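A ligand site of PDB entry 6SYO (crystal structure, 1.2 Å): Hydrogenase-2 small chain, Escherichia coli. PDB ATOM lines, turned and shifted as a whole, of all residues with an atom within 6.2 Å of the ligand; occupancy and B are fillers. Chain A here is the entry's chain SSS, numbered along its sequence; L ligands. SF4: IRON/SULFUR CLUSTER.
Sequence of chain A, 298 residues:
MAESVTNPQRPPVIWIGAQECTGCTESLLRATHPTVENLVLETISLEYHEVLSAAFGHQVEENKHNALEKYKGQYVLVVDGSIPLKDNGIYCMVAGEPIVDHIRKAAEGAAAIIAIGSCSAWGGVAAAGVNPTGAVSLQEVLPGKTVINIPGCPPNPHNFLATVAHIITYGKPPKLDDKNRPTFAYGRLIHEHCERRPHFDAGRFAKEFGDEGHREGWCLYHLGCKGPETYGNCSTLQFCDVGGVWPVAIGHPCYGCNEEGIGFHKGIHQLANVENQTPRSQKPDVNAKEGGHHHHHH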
ATOM      1  N   ILE A 190     -19.494 -22.784  12.792  1.00  0.00           N
ATOM      2  CA  ILE A 190     -18.779 -22.220  11.612  1.00  0.00           C
ATOM      3  C   ILE A 190     -17.291 -22.567  11.720  1.00  0.00           C
ATOM      4  O   ILE A 190     -16.683 -23.036  10.686  1.00  0.00           O
ATOM      5  CB  ILE A 190     -19.070 -20.711  11.440  1.00  0.00           C
ATOM      6  CG1 ILE A 190     -20.554 -20.509  11.021  1.00  0.00           C
ATOM      7  CG2 ILE A 190     -18.126 -20.080  10.438  1.00  0.00           C
ATOM      8  CD1 ILE A 190     -21.014 -19.053  11.149  1.00  0.00           C
ATOM      9  N   HIS A 191     -16.650 -22.430  12.898  1.00  0.00           N
ATOM     10  CA  HIS A 191     -15.207 -22.708  13.066  1.00  0.00           C
ATOM     11  C   HIS A 191     -14.883 -24.219  12.899  1.00  0.00           C
ATOM     12  O   HIS A 191     -13.671 -24.503  12.664  1.00  0.00           O
ATOM     13  CB  HIS A 191     -14.821 -22.203  14.473  1.00  0.00           C
ATOM     14  CG  HIS A 191     -13.404 -22.364  14.923  1.00  0.00           C
ATOM     15  ND1 HIS A 191     -12.359 -21.538  14.448  1.00  0.00           N
ATOM     16  CD2 HIS A 191     -12.831 -23.230  15.802  1.00  0.00           C
ATOM     17  CE1 HIS A 191     -11.229 -21.924  15.092  1.00  0.00           C
ATOM     18  NE2 HIS A 191     -11.482 -22.955  15.905  1.00  0.00           N
ATOM     19  N   GLU A 192     -15.841 -25.090  13.050  1.00  0.00           N
ATOM     20  CA  GLU A 192     -15.618 -26.523  12.799  1.00  0.00           C
ATOM     21  C   GLU A 192     -15.859 -26.918  11.317  1.00  0.00           C
ATOM     22  O   GLU A 192     -15.796 -28.143  10.970  1.00  0.00           O
ATOM     23  CB  GLU A 192     -16.440 -27.389  13.779  1.00  0.00           C
ATOM     24  CG  GLU A 192     -15.953 -27.202  15.240  1.00  0.00           C
ATOM     25  CD  GLU A 192     -14.478 -27.570  15.472  1.00  0.00           C
ATOM     26  OE1 GLU A 192     -13.683 -26.758  16.007  1.00  0.00           O
ATOM     27  OE2 GLU A 192     -14.059 -28.657  15.033  1.00  0.00           O
ATOM     28  N   CYS A 194     -14.543 -24.235   8.673  1.00  0.00           N
ATOM     29  CA  CYS A 194     -14.022 -22.965   8.096  1.00  0.00           C
ATOM     30  C   CYS A 194     -12.712 -23.182   7.342  1.00  0.00           C
ATOM     31  O   CYS A 194     -11.756 -23.774   7.918  1.00  0.00           O
ATOM     32  CB  CYS A 194     -13.814 -21.916   9.197  1.00  0.00           C
ATOM     33  SG  CYS A 194     -13.171 -20.317   8.524  1.00  0.00           S
ATOM     34  N   GLU A 195     -12.609 -22.692   6.119  1.00  0.00           N
ATOM     35  CA  GLU A 195     -11.423 -22.851   5.278  1.00  0.00           C
ATOM     36  C   GLU A 195     -10.185 -22.088   5.808  1.00  0.00           C
ATOM     37  O   GLU A 195      -9.063 -22.357   5.294  1.00  0.00           O
ATOM     38  CB  GLU A 195     -11.730 -22.489   3.818  1.00  0.00           C
ATOM     39  CG  GLU A 195     -12.042 -21.005   3.543  1.00  0.00           C
ATOM     40  CD  GLU A 195     -13.455 -20.462   3.784  1.00  0.00           C
ATOM     41  OE1 GLU A 195     -14.311 -21.115   4.455  1.00  0.00           O
ATOM     42  OE2 GLU A 195     -13.701 -19.270   3.250  1.00  0.00           O
ATOM     43  N   ARG A 196     -10.354 -21.186   6.804  1.00  0.00           N
ATOM     44  CA  ARG A 196      -9.193 -20.499   7.399  1.00  0.00           C
ATOM     45  C   ARG A 196      -8.705 -21.267   8.653  1.00  0.00           C
ATOM     46  O   ARG A 196      -7.675 -20.799   9.222  1.00  0.00           O
ATOM     47  CB  ARG A 196      -9.473 -19.038   7.670  1.00  0.00           C
ATOM     48  CG  ARG A 196      -9.924 -18.307   6.407  1.00  0.00           C
ATOM     49  CD  ARG A 196      -9.896 -16.808   6.467  1.00  0.00           C
ATOM     50  NE  ARG A 196     -10.235 -16.240   5.159  1.00  0.00           N
ATOM     51  CZ  ARG A 196      -9.993 -15.008   4.787  1.00  0.00           C
ATOM     52  NH1 ARG A 196      -9.482 -14.110   5.614  1.00  0.00           N
ATOM     53  NH2 ARG A 196     -10.296 -14.610   3.568  1.00  0.00           N
ATOM     54  N   ARG A 197      -9.256 -22.403   8.981  1.00  0.00           N
ATOM     55  CA  ARG A 197      -8.757 -23.139  10.188  1.00  0.00           C
ATOM     56  C   ARG A 197      -7.266 -23.501  10.058  1.00  0.00           C
ATOM     57  O   ARG A 197      -6.567 -23.453  11.100  1.00  0.00           O
ATOM     58  CB  ARG A 197      -9.608 -24.405  10.379  1.00  0.00           C
ATOM     59  CG  ARG A 197      -9.187 -25.261  11.591  1.00  0.00           C
ATOM     60  CD  ARG A 197      -9.311 -24.542  12.945  1.00  0.00           C
ATOM     61  NE  ARG A 197      -9.053 -25.477  14.044  1.00  0.00           N
ATOM     62  CZ  ARG A 197      -9.988 -26.256  14.596  1.00  0.00           C
ATOM     63  NH1 ARG A 197     -11.280 -26.074  14.365  1.00  0.00           N
ATOM     64  NH2 ARG A 197      -9.589 -27.225  15.436  1.00  0.00           N
ATOM     65  N   PRO A 198      -6.663 -23.828   8.884  1.00  0.00           N
ATOM     66  CA  PRO A 198      -5.219 -24.066   8.856  1.00  0.00           C
ATOM     67  C   PRO A 198      -4.424 -22.870   9.401  1.00  0.00           C
ATOM     68  O   PRO A 198      -3.327 -23.087  10.015  1.00  0.00           O
ATOM     69  CB  PRO A 198      -4.889 -24.337   7.372  1.00  0.00           C
ATOM     70  CG  PRO A 198      -6.228 -24.849   6.793  1.00  0.00           C
ATOM     71  CD  PRO A 198      -7.272 -24.027   7.535  1.00  0.00           C
ATOM     72  N   PHE A 200      -5.488 -20.499  11.589  1.00  0.00           N
ATOM     73  CA  PHE A 200      -5.728 -20.501  13.061  1.00  0.00           C
ATOM     74  C   PHE A 200      -4.722 -21.482  13.667  1.00  0.00           C
ATOM     75  O   PHE A 200      -4.018 -21.131  14.692  1.00  0.00           O
ATOM     76  CB  PHE A 200      -7.180 -20.901  13.355  1.00  0.00           C
ATOM     77  CG  PHE A 200      -7.501 -20.965  14.837  1.00  0.00           C
ATOM     78  CD1 PHE A 200      -7.336 -22.148  15.535  1.00  0.00           C
ATOM     79  CD2 PHE A 200      -8.105 -19.902  15.486  1.00  0.00           C
ATOM     80  CE1 PHE A 200      -7.715 -22.235  16.852  1.00  0.00           C
ATOM     81  CE2 PHE A 200      -8.462 -19.988  16.825  1.00  0.00           C
ATOM     82  CZ  PHE A 200      -8.269 -21.167  17.531  1.00  0.00           C
ATOM     83  N   PHE A 205      -2.429 -14.959  11.790  1.00  0.00           N
ATOM     84  CA  PHE A 205      -3.573 -14.097  12.118  1.00  0.00           C
ATOM     85  C   PHE A 205      -3.431 -12.735  11.468  1.00  0.00           C
ATOM     86  O   PHE A 205      -2.367 -12.072  11.581  1.00  0.00           O
ATOM     87  CB  PHE A 205      -3.729 -13.937  13.654  1.00  0.00           C
ATOM     88  CG  PHE A 205      -3.958 -15.224  14.404  1.00  0.00           C
ATOM     89  CD1 PHE A 205      -5.164 -15.931  14.272  1.00  0.00           C
ATOM     90  CD2 PHE A 205      -3.003 -15.685  15.347  1.00  0.00           C
ATOM     91  CE1 PHE A 205      -5.426 -17.050  15.030  1.00  0.00           C
ATOM     92  CE2 PHE A 205      -3.306 -16.799  16.096  1.00  0.00           C
ATOM     93  CZ  PHE A 205      -4.471 -17.524  15.932  1.00  0.00           C
ATOM     94  N   TRP A 218      -5.497 -14.704   5.846  1.00  0.00           N
ATOM     95  CA  TRP A 218      -5.255 -15.412   7.128  1.00  0.00           C
ATOM     96  C   TRP A 218      -6.466 -15.396   8.056  1.00  0.00           C
ATOM     97  O   TRP A 218      -7.515 -14.708   7.774  1.00  0.00           O
ATOM     98  CB  TRP A 218      -3.989 -14.823   7.799  1.00  0.00           C
ATOM     99  CG  TRP A 218      -2.688 -15.175   7.159  1.00  0.00           C
ATOM    100  CD1 TRP A 218      -2.463 -15.884   6.011  1.00  0.00           C
ATOM    101  CD2 TRP A 218      -1.353 -14.788   7.620  1.00  0.00           C
ATOM    102  NE1 TRP A 218      -1.108 -15.974   5.751  1.00  0.00           N
ATOM    103  CE2 TRP A 218      -0.430 -15.303   6.725  1.00  0.00           C
ATOM    104  CE3 TRP A 218      -0.900 -14.036   8.712  1.00  0.00           C
ATOM    105  CZ2 TRP A 218       0.966 -15.184   6.950  1.00  0.00           C
ATOM    106  CZ3 TRP A 218       0.450 -13.897   8.959  1.00  0.00           C
ATOM    107  CH2 TRP A 218       1.347 -14.446   8.059  1.00  0.00           C
ATOM    108  N   CYS A 219      -6.403 -16.149   9.147  1.00  0.00           N
ATOM    109  CA  CYS A 219      -7.546 -16.282  10.099  1.00  0.00           C
ATOM    110  C   CYS A 219      -7.884 -14.912  10.736  1.00  0.00           C
ATOM    111  O   CYS A 219      -6.949 -14.105  11.010  1.00  0.00           O
ATOM    112  CB  CYS A 219      -7.222 -17.374  11.136  1.00  0.00           C
ATOM    113  SG  CYS A 219      -8.340 -17.416  12.585  1.00  0.00           S
ATOM    114  N   LEU A 220      -9.184 -14.649  10.960  1.00  0.00           N
ATOM    115  CA  LEU A 220      -9.718 -13.392  11.508  1.00  0.00           C
ATOM    116  C   LEU A 220     -10.012 -13.463  13.044  1.00  0.00           C
ATOM    117  O   LEU A 220     -10.682 -12.547  13.596  1.00  0.00           O
ATOM    118  CB  LEU A 220     -10.936 -12.978  10.684  1.00  0.00           C
ATOM    119  CG  LEU A 220     -10.689 -12.915   9.164  1.00  0.00           C
ATOM    120  CD1 LEU A 220     -11.940 -12.313   8.475  1.00  0.00           C
ATOM    121  CD2 LEU A 220      -9.468 -12.079   8.786  1.00  0.00           C
ATOM    122  N   TYR A 221      -9.555 -14.520  13.748  1.00  0.00           N
ATOM    123  CA  TYR A 221      -9.837 -14.710  15.195  1.00  0.00           C
ATOM    124  C   TYR A 221      -9.499 -13.423  15.997  1.00  0.00           C
ATOM    125  O   TYR A 221     -10.322 -12.978  16.857  1.00  0.00           O
ATOM    126  CB  TYR A 221      -9.096 -15.907  15.800  1.00  0.00           C
ATOM    127  CG  TYR A 221      -9.374 -16.091  17.281  1.00  0.00           C
ATOM    128  CD1 TYR A 221     -10.589 -16.576  17.717  1.00  0.00           C
ATOM    129  CD2 TYR A 221      -8.453 -15.674  18.248  1.00  0.00           C
ATOM    130  CE1 TYR A 221     -10.917 -16.659  19.064  1.00  0.00           C
ATOM    131  CE2 TYR A 221      -8.767 -15.728  19.594  1.00  0.00           C
ATOM    132  CZ  TYR A 221      -9.993 -16.209  20.013  1.00  0.00           C
ATOM    133  OH  TYR A 221     -10.299 -16.224  21.377  1.00  0.00           O
ATOM    134  N   CYS A 225     -13.494 -12.605  15.322  1.00  0.00           N
ATOM    135  CA  CYS A 225     -14.352 -13.630  14.657  1.00  0.00           C
ATOM    136  C   CYS A 225     -15.120 -14.447  15.690  1.00  0.00           C
ATOM    137  O   CYS A 225     -14.514 -15.103  16.595  1.00  0.00           O
ATOM    138  CB  CYS A 225     -13.517 -14.497  13.733  1.00  0.00           C
ATOM    139  SG  CYS A 225     -14.573 -15.598  12.710  1.00  0.00           S
ATOM    140  N   LYS A 226     -16.442 -14.566  15.504  1.00  0.00           N
ATOM    141  CA  LYS A 226     -17.333 -15.332  16.385  1.00  0.00           C
ATOM    142  C   LYS A 226     -17.645 -16.742  15.849  1.00  0.00           C
ATOM    143  O   LYS A 226     -18.440 -17.486  16.431  1.00  0.00           O
ATOM    144  CB  LYS A 226     -18.619 -14.587  16.723  1.00  0.00           C
ATOM    145  CG  LYS A 226     -18.390 -13.184  17.311  1.00  0.00           C
ATOM    146  CD  LYS A 226     -17.444 -13.127  18.527  1.00  0.00           C
ATOM    147  CE  LYS A 226     -17.439 -11.813  19.307  1.00  0.00           C
ATOM    148  NZ  LYS A 226     -17.086 -10.673  18.374  1.00  0.00           N
ATOM    149  N   GLY A 227     -16.961 -17.155  14.770  1.00  0.00           N
ATOM    150  CA  GLY A 227     -17.098 -18.541  14.238  1.00  0.00           C
ATOM    151  C   GLY A 227     -16.963 -19.650  15.305  1.00  0.00           C
ATOM    152  O   GLY A 227     -17.707 -20.637  15.274  1.00  0.00           O
ATOM    153  N   PRO A 228     -16.051 -19.488  16.304  1.00  0.00           N
ATOM    154  CA  PRO A 228     -15.921 -20.532  17.344  1.00  0.00           C
ATOM    155  C   PRO A 228     -17.126 -20.758  18.248  1.00  0.00           C
ATOM    156  O   PRO A 228     -17.213 -21.802  18.951  1.00  0.00           O
ATOM    157  CB  PRO A 228     -14.685 -20.093  18.163  1.00  0.00           C
ATOM    158  CG  PRO A 228     -13.867 -19.277  17.183  1.00  0.00           C
ATOM    159  CD  PRO A 228     -14.933 -18.537  16.354  1.00  0.00           C
ATOM    160  N   TRP A 246     -19.021 -14.908   1.598  1.00  0.00           N
ATOM    161  CA  TRP A 246     -19.520 -14.843   2.985  1.00  0.00           C
ATOM    162  C   TRP A 246     -18.657 -13.854   3.734  1.00  0.00           C
ATOM    163  O   TRP A 246     -17.595 -13.407   3.166  1.00  0.00           O
ATOM    164  CB  TRP A 246     -19.580 -16.241   3.669  1.00  0.00           C
ATOM    165  CG  TRP A 246     -18.267 -16.921   4.029  1.00  0.00           C
ATOM    166  CD1 TRP A 246     -17.340 -17.503   3.198  1.00  0.00           C
ATOM    167  CD2 TRP A 246     -17.820 -17.241   5.398  1.00  0.00           C
ATOM    168  NE1 TRP A 246     -16.362 -18.164   3.936  1.00  0.00           N
ATOM    169  CE2 TRP A 246     -16.613 -18.003   5.277  1.00  0.00           C
ATOM    170  CE3 TRP A 246     -18.328 -16.978   6.688  1.00  0.00           C
ATOM    171  CZ2 TRP A 246     -15.933 -18.527   6.403  1.00  0.00           C
ATOM    172  CZ3 TRP A 246     -17.685 -17.491   7.780  1.00  0.00           C
ATOM    173  CH2 TRP A 246     -16.519 -18.270   7.620  1.00  0.00           C
ATOM    174  N   VAL A 248     -16.372 -13.687   6.173  1.00  0.00           N
ATOM    175  CA  VAL A 248     -14.940 -14.003   6.411  1.00  0.00           C
ATOM    176  C   VAL A 248     -14.210 -14.037   5.079  1.00  0.00           C
ATOM    177  O   VAL A 248     -13.079 -13.478   4.937  1.00  0.00           O
ATOM    178  CB  VAL A 248     -14.795 -15.307   7.197  1.00  0.00           C
ATOM    179  CG1 VAL A 248     -13.373 -15.867   7.117  1.00  0.00           C
ATOM    180  CG2 VAL A 248     -15.193 -15.093   8.660  1.00  0.00           C
ATOM    181  N   CYS A 254     -16.823 -13.015  11.374  1.00  0.00           N
ATOM    182  CA  CYS A 254     -18.192 -13.296  11.819  1.00  0.00           C
ATOM    183  C   CYS A 254     -18.528 -12.523  13.093  1.00  0.00           C
ATOM    184  O   CYS A 254     -17.622 -12.420  14.006  1.00  0.00           O
ATOM    185  CB  CYS A 254     -18.345 -14.843  12.021  1.00  0.00           C
ATOM    186  SG  CYS A 254     -19.943 -15.384  12.760  1.00  0.00           S
HETATM  187 FE1  SF4 L   1     -10.443 -18.214  12.039  1.00  0.00          FE
HETATM  188 FE2  SF4 L   1     -13.127 -17.374  12.286  1.00  0.00          FE
HETATM  189 FE3  SF4 L   1     -12.328 -19.899  13.129  1.00  0.00          FE
HETATM  190 FE4  SF4 L   1     -12.437 -19.314  10.470  1.00  0.00          FE
HETATM  191  S1  SF4 L   1     -14.255 -19.392  11.981  1.00  0.00           S
HETATM  192  S2  SF4 L   1     -10.703 -20.451  11.530  1.00  0.00           S
HETATM  193  S3  SF4 L   1     -11.691 -17.115  10.425  1.00  0.00           S
HETATM  194  S4  SF4 L   1     -11.684 -17.875  14.028  1.00  0.00           S
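Arg 196 touches the ligand.
Phe 200 touches the ligand.
CB of Tyr 221 touches S4 of the ligand, 3.7 Å away.
Gly 227 touches the ligand (CA to S1, 3.7 Å).
Val 248 touches the ligand.
Hydrophobic or aromatic side chains that line the ligand: His 191, Phe 200, Tyr 221 and Val 248.
Along chain A the residues within 4 Å of the ligand span positions 191 to 248.
The nearest printed residue that does not touch the ligand is Pro 228 (4.1 Å).
SG of Cys 225 sits close to N of Cys 254 (3.7 Å).
N of His 191 sits at hydrogen-bond distance from O of Gly 227, at 3.2 Å.
NH2 of Arg 196 lies within hydrogen-bond range of O of Val 248.
N of Arg 196 sits close to SG of Cys 194.
The backbone carbonyl oxygen of Trp 218 is in hydrogen-bond range of the guanidinium group of Arg 196 (3.0 Å).
The side-chain carboxylate (OE1) of Glu 192 is in salt-bridge range of the guanidinium group (NH1) of Arg 197 (3.0 Å).
The side-chain sulfur of Cys 225 sits close to the backbone NH of Gly 227 (3.5 Å).
N of Tyr 221 sits close to SG of Cys 219, 3.3 Å away.
The side-chain sulfur of Cys 225 is bound to an iron atom (FE2) of the ligand (2.3 Å).
A sulfur (S3) of the ligand lies close to the backbone NH (N) of Leu 220, at 3.6 Å.
The side-chain sulfur (SG) of Cys 219 is bound to an iron atom (FE1) of the ligand, 2.3 Å away.
A ring nitrogen (ND1) of His 191 is bound to an iron atom (FE3) of the ligand, 2.1 Å away.
N of Arg 197 sits close to S2 of the ligand, at 3.5 Å.
The side-chain sulfur (SG) of Cys 194 binds an iron atom (FE4) of the ligand (2.3 Å).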
